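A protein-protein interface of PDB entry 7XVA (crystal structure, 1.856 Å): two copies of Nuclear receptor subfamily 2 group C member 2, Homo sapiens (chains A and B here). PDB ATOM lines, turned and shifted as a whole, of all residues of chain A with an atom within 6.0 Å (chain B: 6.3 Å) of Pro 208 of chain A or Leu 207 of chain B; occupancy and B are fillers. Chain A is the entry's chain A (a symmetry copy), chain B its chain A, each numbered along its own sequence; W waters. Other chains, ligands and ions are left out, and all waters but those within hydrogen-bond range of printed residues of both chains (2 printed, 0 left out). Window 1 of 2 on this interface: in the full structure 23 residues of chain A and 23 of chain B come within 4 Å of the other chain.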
ATOM      1  N   LEU A 204      13.206   5.482 -22.491  1.00  0.00           N
ATOM      2  CA  LEU A 204      13.583   4.250 -21.761  1.00  0.00           C
ATOM      3  C   LEU A 204      14.980   3.759 -22.161  1.00  0.00           C
ATOM      4  O   LEU A 204      15.689   3.170 -21.308  1.00  0.00           O
ATOM      5  CB  LEU A 204      12.528   3.184 -22.018  1.00  0.00           C
ATOM      6  CG  LEU A 204      11.165   3.512 -21.430  1.00  0.00           C
ATOM      7  CD1 LEU A 204      10.183   2.424 -21.800  1.00  0.00           C
ATOM      8  CD2 LEU A 204      11.275   3.670 -19.919  1.00  0.00           C
ATOM      9  N   VAL A 205      15.403   4.001 -23.392  1.00  0.00           N
ATOM     10  CA  VAL A 205      16.754   3.555 -23.846  1.00  0.00           C
ATOM     11  C   VAL A 205      17.857   4.472 -23.273  1.00  0.00           C
ATOM     12  O   VAL A 205      19.031   4.158 -23.464  1.00  0.00           O
ATOM     13  CB  VAL A 205      16.783   3.452 -25.376  1.00  0.00           C
ATOM     14  CG1 VAL A 205      18.194   3.177 -25.907  1.00  0.00           C
ATOM     15  CG2 VAL A 205      15.835   2.361 -25.835  1.00  0.00           C
ATOM     16  N   ARG A 206      17.522   5.479 -22.475  1.00  0.00           N
ATOM     17  CA  ARG A 206      18.526   6.260 -21.690  1.00  0.00           C
ATOM     18  C   ARG A 206      18.909   5.568 -20.378  1.00  0.00           C
ATOM     19  O   ARG A 206      19.992   5.850 -19.873  1.00  0.00           O
ATOM     20  CB  ARG A 206      17.978   7.650 -21.366  1.00  0.00           C
ATOM     21  CG  ARG A 206      17.721   8.468 -22.624  1.00  0.00           C
ATOM     22  CD  ARG A 206      18.945   9.093 -23.261  1.00  0.00           C
ATOM     23  NE  ARG A 206      19.837   8.131 -23.878  1.00  0.00           N
ATOM     24  CZ  ARG A 206      21.119   7.901 -23.526  1.00  0.00           C
ATOM     25  NH1 ARG A 206      21.716   8.581 -22.558  1.00  0.00           N
ATOM     26  NH2 ARG A 206      21.794   6.943 -24.137  1.00  0.00           N
ATOM     27  N   LEU A 207      18.038   4.709 -19.855  1.00  0.00           N
ATOM     28  CA  LEU A 207      18.191   4.108 -18.508  1.00  0.00           C
ATOM     29  C   LEU A 207      19.452   3.262 -18.449  1.00  0.00           C
ATOM     30  O   LEU A 207      20.097   3.314 -17.414  1.00  0.00           O
ATOM     31  CB  LEU A 207      16.964   3.282 -18.108  1.00  0.00           C
ATOM     32  CG  LEU A 207      15.739   4.120 -17.745  1.00  0.00           C
ATOM     33  CD1 LEU A 207      14.522   3.263 -17.459  1.00  0.00           C
ATOM     34  CD2 LEU A 207      16.007   5.056 -16.584  1.00  0.00           C
ATOM     35  N   PRO A 208      19.829   2.464 -19.476  1.00  0.00           N
ATOM     36  CA  PRO A 208      21.048   1.668 -19.375  1.00  0.00           C
ATOM     37  C   PRO A 208      22.295   2.526 -19.135  1.00  0.00           C
ATOM     38  O   PRO A 208      23.250   2.048 -18.564  1.00  0.00           O
ATOM     39  CB  PRO A 208      21.120   0.925 -20.725  1.00  0.00           C
ATOM     40  CG  PRO A 208      19.660   0.848 -21.202  1.00  0.00           C
ATOM     41  CD  PRO A 208      19.066   2.149 -20.697  1.00  0.00           C
ATOM     42  N   ALA A 209      22.304   3.775 -19.604  1.00  0.00           N
ATOM     43  CA  ALA A 209      23.478   4.656 -19.457  1.00  0.00           C
ATOM     44  C   ALA A 209      23.792   4.831 -17.971  1.00  0.00           C
ATOM     45  O   ALA A 209      24.982   4.935 -17.625  1.00  0.00           O
ATOM     46  CB  ALA A 209      23.228   5.968 -20.176  1.00  0.00           C
ATOM     47  N   LEU A 210      22.794   4.801 -17.086  1.00  0.00           N
ATOM     48  CA  LEU A 210      23.029   5.052 -15.639  1.00  0.00           C
ATOM     49  C   LEU A 210      23.916   3.954 -15.055  1.00  0.00           C
ATOM     50  O   LEU A 210      24.727   4.223 -14.098  1.00  0.00           O
ATOM     51  CB  LEU A 210      21.675   5.068 -14.930  1.00  0.00           C
ATOM     52  CG  LEU A 210      20.747   6.215 -15.313  1.00  0.00           C
ATOM     53  CD1 LEU A 210      19.398   6.012 -14.698  1.00  0.00           C
ATOM     54  CD2 LEU A 210      21.320   7.544 -14.840  1.00  0.00           C
ATOM     55  N   ARG A 211      23.782   2.729 -15.578  1.00  0.00           N
ATOM     56  CA  ARG A 211      24.529   1.577 -15.025  1.00  0.00           C
ATOM     57  C   ARG A 211      25.936   1.476 -15.603  1.00  0.00           C
ATOM     58  O   ARG A 211      26.692   0.617 -15.140  1.00  0.00           O
ATOM     59  CB  ARG A 211      23.666   0.337 -15.225  1.00  0.00           C
ATOM     60  CG  ARG A 211      22.488   0.403 -14.276  1.00  0.00           C
ATOM     61  CD  ARG A 211      21.718  -0.866 -14.166  1.00  0.00           C
ATOM     62  NE  ARG A 211      20.680  -0.832 -13.151  1.00  0.00           N
ATOM     63  CZ  ARG A 211      19.775  -1.800 -13.029  1.00  0.00           C
ATOM     64  NH1 ARG A 211      19.812  -2.815 -13.869  1.00  0.00           N
ATOM     65  NH2 ARG A 211      18.842  -1.760 -12.097  1.00  0.00           N
ATOM     66  N   LEU A 212      26.300   2.324 -16.548  1.00  0.00           N
ATOM     67  CA  LEU A 212      27.681   2.396 -17.060  1.00  0.00           C
ATOM     68  C   LEU A 212      28.527   3.293 -16.146  1.00  0.00           C
ATOM     69  O   LEU A 212      29.773   3.363 -16.347  1.00  0.00           O
ATOM     70  CB  LEU A 212      27.597   2.890 -18.506  1.00  0.00           C
ATOM     71  CG  LEU A 212      28.491   2.189 -19.523  1.00  0.00           C
ATOM     72  CD1 LEU A 212      28.380   0.676 -19.423  1.00  0.00           C
ATOM     73  CD2 LEU A 212      28.173   2.689 -20.920  1.00  0.00           C
ATOM     74  N   GLU B  85      27.135  -7.684 -23.359  1.00  0.00           N
ATOM     75  CA  GLU B  85      25.661  -7.469 -23.448  1.00  0.00           C
ATOM     76  C   GLU B  85      25.080  -8.320 -24.596  1.00  0.00           C
ATOM     77  O   GLU B  85      24.033  -8.930 -24.405  1.00  0.00           O
ATOM     78  CB  GLU B  85      25.353  -5.977 -23.635  1.00  0.00           C
ATOM     79  CG  GLU B  85      25.916  -5.102 -22.518  1.00  0.00           C
ATOM     80  CD  GLU B  85      25.691  -3.612 -22.755  1.00  0.00           C
ATOM     81  OE1 GLU B  85      24.517  -3.243 -23.063  1.00  0.00           O
ATOM     82  OE2 GLU B  85      26.682  -2.805 -22.623  1.00  0.00           O
ATOM     83  N   LEU B  89      22.405 -11.389 -24.071  1.00  0.00           N
ATOM     84  CA  LEU B  89      21.110 -11.495 -24.775  1.00  0.00           C
ATOM     85  C   LEU B  89      21.050 -12.866 -25.474  1.00  0.00           C
ATOM     86  O   LEU B  89      19.973 -13.459 -25.524  1.00  0.00           O
ATOM     87  CB  LEU B  89      20.971 -10.347 -25.786  1.00  0.00           C
ATOM     88  CG  LEU B  89      20.483  -9.054 -25.139  1.00  0.00           C
ATOM     89  CD1 LEU B  89      20.701  -7.901 -26.058  1.00  0.00           C
ATOM     90  CD2 LEU B  89      19.028  -9.161 -24.740  1.00  0.00           C
ATOM     91  N   PHE B 138      17.970 -12.816 -15.231  1.00  0.00           N
ATOM     92  CA  PHE B 138      17.826 -12.171 -16.559  1.00  0.00           C
ATOM     93  C   PHE B 138      17.174 -13.157 -17.531  1.00  0.00           C
ATOM     94  O   PHE B 138      16.116 -12.833 -18.108  1.00  0.00           O
ATOM     95  CB  PHE B 138      19.156 -11.691 -17.104  1.00  0.00           C
ATOM     96  CG  PHE B 138      18.946 -10.943 -18.396  1.00  0.00           C
ATOM     97  CD1 PHE B 138      18.300  -9.724 -18.391  1.00  0.00           C
ATOM     98  CD2 PHE B 138      19.254 -11.531 -19.607  1.00  0.00           C
ATOM     99  CE1 PHE B 138      18.068  -9.037 -19.575  1.00  0.00           C
ATOM    100  CE2 PHE B 138      19.044 -10.834 -20.792  1.00  0.00           C
ATOM    101  CZ  PHE B 138      18.428  -9.604 -20.768  1.00  0.00           C
ATOM    102  N   LEU B 155      16.710  -5.894 -29.858  1.00  0.00           N
ATOM    103  CA  LEU B 155      17.409  -5.634 -28.573  1.00  0.00           C
ATOM    104  C   LEU B 155      18.930  -5.677 -28.766  1.00  0.00           C
ATOM    105  O   LEU B 155      19.625  -4.827 -28.177  1.00  0.00           O
ATOM    106  CB  LEU B 155      16.936  -6.619 -27.497  1.00  0.00           C
ATOM    107  CG  LEU B 155      15.478  -6.440 -27.082  1.00  0.00           C
ATOM    108  CD1 LEU B 155      15.055  -7.566 -26.118  1.00  0.00           C
ATOM    109  CD2 LEU B 155      15.259  -5.061 -26.472  1.00  0.00           C
ATOM    110  N   LYS B 156      19.443  -6.631 -29.538  1.00  0.00           N
ATOM    111  CA  LYS B 156      20.901  -6.740 -29.806  1.00  0.00           C
ATOM    112  C   LYS B 156      21.355  -5.505 -30.570  1.00  0.00           C
ATOM    113  O   LYS B 156      22.427  -5.015 -30.319  1.00  0.00           O
ATOM    114  CB  LYS B 156      21.191  -8.026 -30.588  1.00  0.00           C
ATOM    115  CG  LYS B 156      20.964  -9.303 -29.785  1.00  0.00           C
ATOM    116  CD  LYS B 156      21.209 -10.543 -30.618  1.00  0.00           C
ATOM    117  CE  LYS B 156      20.775 -11.764 -29.865  1.00  0.00           C
ATOM    118  NZ  LYS B 156      20.945 -12.933 -30.729  1.00  0.00           N
ATOM    119  N   ILE B 158      20.049  -2.541 -30.489  1.00  0.00           N
ATOM    120  CA  ILE B 158      20.040  -1.381 -29.551  1.00  0.00           C
ATOM    121  C   ILE B 158      21.308  -1.418 -28.683  1.00  0.00           C
ATOM    122  O   ILE B 158      21.938  -0.352 -28.441  1.00  0.00           O
ATOM    123  CB  ILE B 158      18.742  -1.348 -28.717  1.00  0.00           C
ATOM    124  CG1 ILE B 158      17.558  -1.023 -29.616  1.00  0.00           C
ATOM    125  CG2 ILE B 158      18.869  -0.372 -27.549  1.00  0.00           C
ATOM    126  CD1 ILE B 158      16.207  -1.218 -28.978  1.00  0.00           C
ATOM    127  N   VAL B 159      21.740  -2.578 -28.206  1.00  0.00           N
ATOM    128  CA  VAL B 159      22.980  -2.621 -27.364  1.00  0.00           C
ATOM    129  C   VAL B 159      24.231  -2.408 -28.213  1.00  0.00           C
ATOM    130  O   VAL B 159      25.166  -1.799 -27.703  1.00  0.00           O
ATOM    131  CB  VAL B 159      23.095  -3.868 -26.470  1.00  0.00           C
ATOM    132  CG1 VAL B 159      21.819  -4.119 -25.715  1.00  0.00           C
ATOM    133  CG2 VAL B 159      23.534  -5.087 -27.184  1.00  0.00           C
ATOM    134  N   ASP B 164      26.883   5.292 -25.688  1.00  0.00           N
ATOM    135  CA  ASP B 164      27.248   5.604 -24.284  1.00  0.00           C
ATOM    136  C   ASP B 164      28.730   5.293 -24.032  1.00  0.00           C
ATOM    137  O   ASP B 164      29.219   5.686 -23.002  1.00  0.00           O
ATOM    138  CB  ASP B 164      26.421   4.795 -23.270  1.00  0.00           C
ATOM    139  CG  ASP B 164      24.911   4.976 -23.311  1.00  0.00           C
ATOM    140  OD1 ASP B 164      24.441   6.033 -23.802  1.00  0.00           O
ATOM    141  OD2 ASP B 164      24.189   4.036 -22.848  1.00  0.00           O
ATOM    142  N   ILE B 203       9.746  -4.646 -22.359  1.00  0.00           N
ATOM    143  CA  ILE B 203      10.975  -5.200 -22.982  1.00  0.00           C
ATOM    144  C   ILE B 203      12.138  -4.217 -22.792  1.00  0.00           C
ATOM    145  O   ILE B 203      13.233  -4.673 -22.444  1.00  0.00           O
ATOM    146  CB  ILE B 203      10.739  -5.525 -24.465  1.00  0.00           C
ATOM    147  CG1 ILE B 203       9.703  -6.631 -24.657  1.00  0.00           C
ATOM    148  CG2 ILE B 203      12.046  -5.890 -25.111  1.00  0.00           C
ATOM    149  CD1 ILE B 203       9.134  -6.628 -26.085  1.00  0.00           C
ATOM    150  N   LEU B 204      11.950  -2.926 -23.067  1.00  0.00           N
ATOM    151  CA  LEU B 204      13.082  -1.975 -22.990  1.00  0.00           C
ATOM    152  C   LEU B 204      13.615  -1.842 -21.558  1.00  0.00           C
ATOM    153  O   LEU B 204      14.836  -1.613 -21.378  1.00  0.00           O
ATOM    154  CB  LEU B 204      12.632  -0.628 -23.539  1.00  0.00           C
ATOM    155  CG  LEU B 204      12.315  -0.644 -25.026  1.00  0.00           C
ATOM    156  CD1 LEU B 204      11.817   0.720 -25.447  1.00  0.00           C
ATOM    157  CD2 LEU B 204      13.551  -1.052 -25.816  1.00  0.00           C
ATOM    158  N   VAL B 205      12.767  -2.006 -20.554  1.00  0.00           N
ATOM    159  CA  VAL B 205      13.219  -1.895 -19.136  1.00  0.00           C
ATOM    160  C   VAL B 205      13.992  -3.161 -18.705  1.00  0.00           C
ATOM    161  O   VAL B 205      14.529  -3.166 -17.598  1.00  0.00           O
ATOM    162  CB  VAL B 205      12.024  -1.575 -18.230  1.00  0.00           C
ATOM    163  CG1 VAL B 205      12.397  -1.632 -16.744  1.00  0.00           C
ATOM    164  CG2 VAL B 205      11.472  -0.205 -18.573  1.00  0.00           C
ATOM    165  N   ARG B 206      14.183  -4.141 -19.581  1.00  0.00           N
ATOM    166  CA  ARG B 206      15.115  -5.283 -19.329  1.00  0.00           C
ATOM    167  C   ARG B 206      16.570  -4.933 -19.658  1.00  0.00           C
ATOM    168  O   ARG B 206      17.455  -5.581 -19.109  1.00  0.00           O
ATOM    169  CB  ARG B 206      14.703  -6.494 -20.167  1.00  0.00           C
ATOM    170  CG  ARG B 206      13.322  -7.008 -19.785  1.00  0.00           C
ATOM    171  CD  ARG B 206      13.259  -7.848 -18.527  1.00  0.00           C
ATOM    172  NE  ARG B 206      13.489  -7.095 -17.310  1.00  0.00           N
ATOM    173  CZ  ARG B 206      14.498  -7.292 -16.436  1.00  0.00           C
ATOM    174  NH1 ARG B 206      15.397  -8.250 -16.604  1.00  0.00           N
ATOM    175  NH2 ARG B 206      14.620  -6.482 -15.399  1.00  0.00           N
ATOM    176  N   LEU B 207      16.787  -3.952 -20.531  1.00  0.00           N
ATOM    177  CA  LEU B 207      18.127  -3.628 -21.079  1.00  0.00           C
ATOM    178  C   LEU B 207      19.061  -3.192 -19.963  1.00  0.00           C
ATOM    179  O   LEU B 207      20.217  -3.578 -20.036  1.00  0.00           O
ATOM    180  CB  LEU B 207      18.052  -2.561 -22.175  1.00  0.00           C
ATOM    181  CG  LEU B 207      17.481  -3.064 -23.500  1.00  0.00           C
ATOM    182  CD1 LEU B 207      17.328  -1.952 -24.518  1.00  0.00           C
ATOM    183  CD2 LEU B 207      18.295  -4.202 -24.081  1.00  0.00           C
ATOM    184  N   PRO B 208      18.648  -2.387 -18.956  1.00  0.00           N
ATOM    185  CA  PRO B 208      19.580  -1.991 -17.905  1.00  0.00           C
ATOM    186  C   PRO B 208      20.174  -3.192 -17.161  1.00  0.00           C
ATOM    187  O   PRO B 208      21.263  -3.094 -16.639  1.00  0.00           O
ATOM    188  CB  PRO B 208      18.734  -1.104 -16.970  1.00  0.00           C
ATOM    189  CG  PRO B 208      17.618  -0.548 -17.872  1.00  0.00           C
ATOM    190  CD  PRO B 208      17.355  -1.689 -18.835  1.00  0.00           C
ATOM    191  N   ALA B 209      19.447  -4.307 -17.076  1.00  0.00           N
ATOM    192  CA  ALA B 209      19.922  -5.495 -16.341  1.00  0.00           C
ATOM    193  C   ALA B 209      21.237  -5.974 -16.955  1.00  0.00           C
ATOM    194  O   ALA B 209      22.100  -6.459 -16.203  1.00  0.00           O
ATOM    195  CB  ALA B 209      18.841  -6.559 -16.334  1.00  0.00           C
ATOM    196  N   LEU B 210      21.450  -5.797 -18.260  1.00  0.00           N
ATOM    197  CA  LEU B 210      22.672  -6.319 -18.928  1.00  0.00           C
ATOM    198  C   LEU B 210      23.911  -5.617 -18.375  1.00  0.00           C
ATOM    199  O   LEU B 210      25.027  -6.244 -18.301  1.00  0.00           O
ATOM    200  CB  LEU B 210      22.546  -6.060 -20.429  1.00  0.00           C
ATOM    201  CG  LEU B 210      21.435  -6.827 -21.136  1.00  0.00           C
ATOM    202  CD1 LEU B 210      21.297  -6.347 -22.547  1.00  0.00           C
ATOM    203  CD2 LEU B 210      21.738  -8.320 -21.141  1.00  0.00           C
ATOM    204  N   ARG B 211      23.763  -4.339 -18.002  1.00  0.00           N
ATOM    205  CA  ARG B 211      24.920  -3.542 -17.537  1.00  0.00           C
ATOM    206  C   ARG B 211      25.203  -3.755 -16.054  1.00  0.00           C
ATOM    207  O   ARG B 211      26.210  -3.224 -15.574  1.00  0.00           O
ATOM    208  CB  ARG B 211      24.664  -2.094 -17.935  1.00  0.00           C
ATOM    209  CG  ARG B 211      24.809  -1.967 -19.438  1.00  0.00           C
ATOM    210  CD  ARG B 211      24.859  -0.564 -19.932  1.00  0.00           C
ATOM    211  NE  ARG B 211      25.138  -0.457 -21.354  1.00  0.00           N
ATOM    212  CZ  ARG B 211      25.044   0.697 -22.010  1.00  0.00           C
ATOM    213  NH1 ARG B 211      24.669   1.774 -21.351  1.00  0.00           N
ATOM    214  NH2 ARG B 211      25.309   0.782 -23.300  1.00  0.00           N
HETATM  215  O   HOH W   1      21.681   3.690 -22.860  1.00  0.00           O
HETATM  216  O   HOH W   2      24.551   8.727 -22.262  1.00  0.00           O
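NH2 of Arg 206 of chain A is in salt-bridge range of OD1 of Asp 164 of chain B, at 2.8 Å.
The guanidinium group of Arg 211 of chain A lies within hydrogen-bond range of the backbone carbonyl oxygen of Pro 208 of chain B (3.1 Å).
O of Pro 208 of chain A lies within hydrogen-bond range of NH1 of Arg 211 of chain B, 3.1 Å away.
The guanidinium group of Arg 211 of chain B lies within salt-bridge range of the side-chain carboxylate of Glu 85 of chain B.
NH1 of Arg 211 of chain B is in salt-bridge range of OD2 of Asp 164 of chain B (2.8 Å).
Among the printed residues, pairs that only touch across the chains: Val 205 of chain A with Ile 158 of chain B (3.97 Å), Leu 207 of chain A with Pro 208 of chain B (3.9 Å), Pro 208 of chain A with Leu 207 of chain B (3.9 Å), Ala 209 of chain A with Asp 164 of chain B (3.4 Å), Ala 209 of chain A with Arg 211 of chain B (3.6 Å), Arg 211 of chain A with Ala 209 of chain B (3.6 Å), Arg 211 of chain A with Arg 211 of chain B (3.8 Å), Leu 212 of chain A with Asp 164 of chain B (3.6 Å) and Leu 212 of chain A with Arg 211 of chain B (3.6 Å).
Printed residues of chain B within 4 Å of Pro 208 of chain A: Leu 207 (3.9 Å) and Arg 211 (3.1 Å).
Of chain A, only Pro 208 (3.9 Å) comes within 4 Å of Leu 207 of chain B.
Of the printed residues of chain B, Leu 212 of chain A touches Asp 164 and Arg 211.
Printed residues of chain B within 4 Å of Arg 211 of chain A: Pro 208 (3.1 Å), Ala 209 (3.6 Å) and Arg 211 (3.8 Å).
Lys 156 of chain B touches none of the printed residues of chain A.
The nearest residue of chain B that does not touch Pro 208 of chain A is Pro 208 of chain B (4.1 Å).
The nearest residue of chain A that does not touch Leu 207 of chain B is Val 205 of chain A (4.8 Å).
The nearest printed residue of chain B that does not touch Leu 212 of chain A is Glu 85 of chain B (5.0 Å).
Of the 17 printed residues of chain B, 6 touch a printed residue of chain A.
Hydrophobic or aromatic side chains of chain B within 4 Å of the printed part of chain A: Ile 158, Leu 207 and Pro 208.
Along chain B the printed residues that touch a printed residue of chain A span positions 158 to 211.
Of the 9 printed residues of chain A, 7 touch a printed residue of chain B.
Hydrophobic or aromatic side chains of chain A that line the printed part of chain B: Val 205, Leu 207, Pro 208, Ala 209 and Leu 212.
Among the printed residues, 12 pairs touch across the chains.
Among the printed residues, Asp or Glu carboxylates within 4 Å of a Lys or Arg side-chain nitrogen of the other chain: Arg 206 of chain A with Asp 164 of chain B (2.8 Å).
Leu 207 of chain A touches Pro 208 of chain B, and with the chains exchanged Pro 208 of chain A touches Leu 207 of chain B.
Pro 208 of chain A touches Arg 211 of chain B, and with the chains exchanged Arg 211 of chain A touches Pro 208 of chain B.
Ala 209 of chain A touches Arg 211 of chain B, and with the chains exchanged Arg 211 of chain A touches Ala 209 of chain B.
Arg 211 of chain A touches its own counterpart, Arg 211 of chain B.
Positions printed for both chains: 204, 205, 206, 207, 208, 209, 210 and 211.
Of the 12 pairs that touch across the chains among the printed residues, 7 have their exchanged pair printed and touching as well.
Water W1 lies within hydrogen-bond range of the side-chain carboxylate (OD2) of Asp 164 of chain B (2.5 Å), the backbone carbonyl oxygen (O) of Val 205 of chain A (2.8 Å), the backbone NH (N) of Ala 209 of chain A (3.3 Å) and the guanidinium group (NH2) of Arg 206 of chain A (3.5 Å).
Water W2 bridges the guanidinium group of Arg 206 of chain A and the side-chain carboxylate of Asp 164 of chain B.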
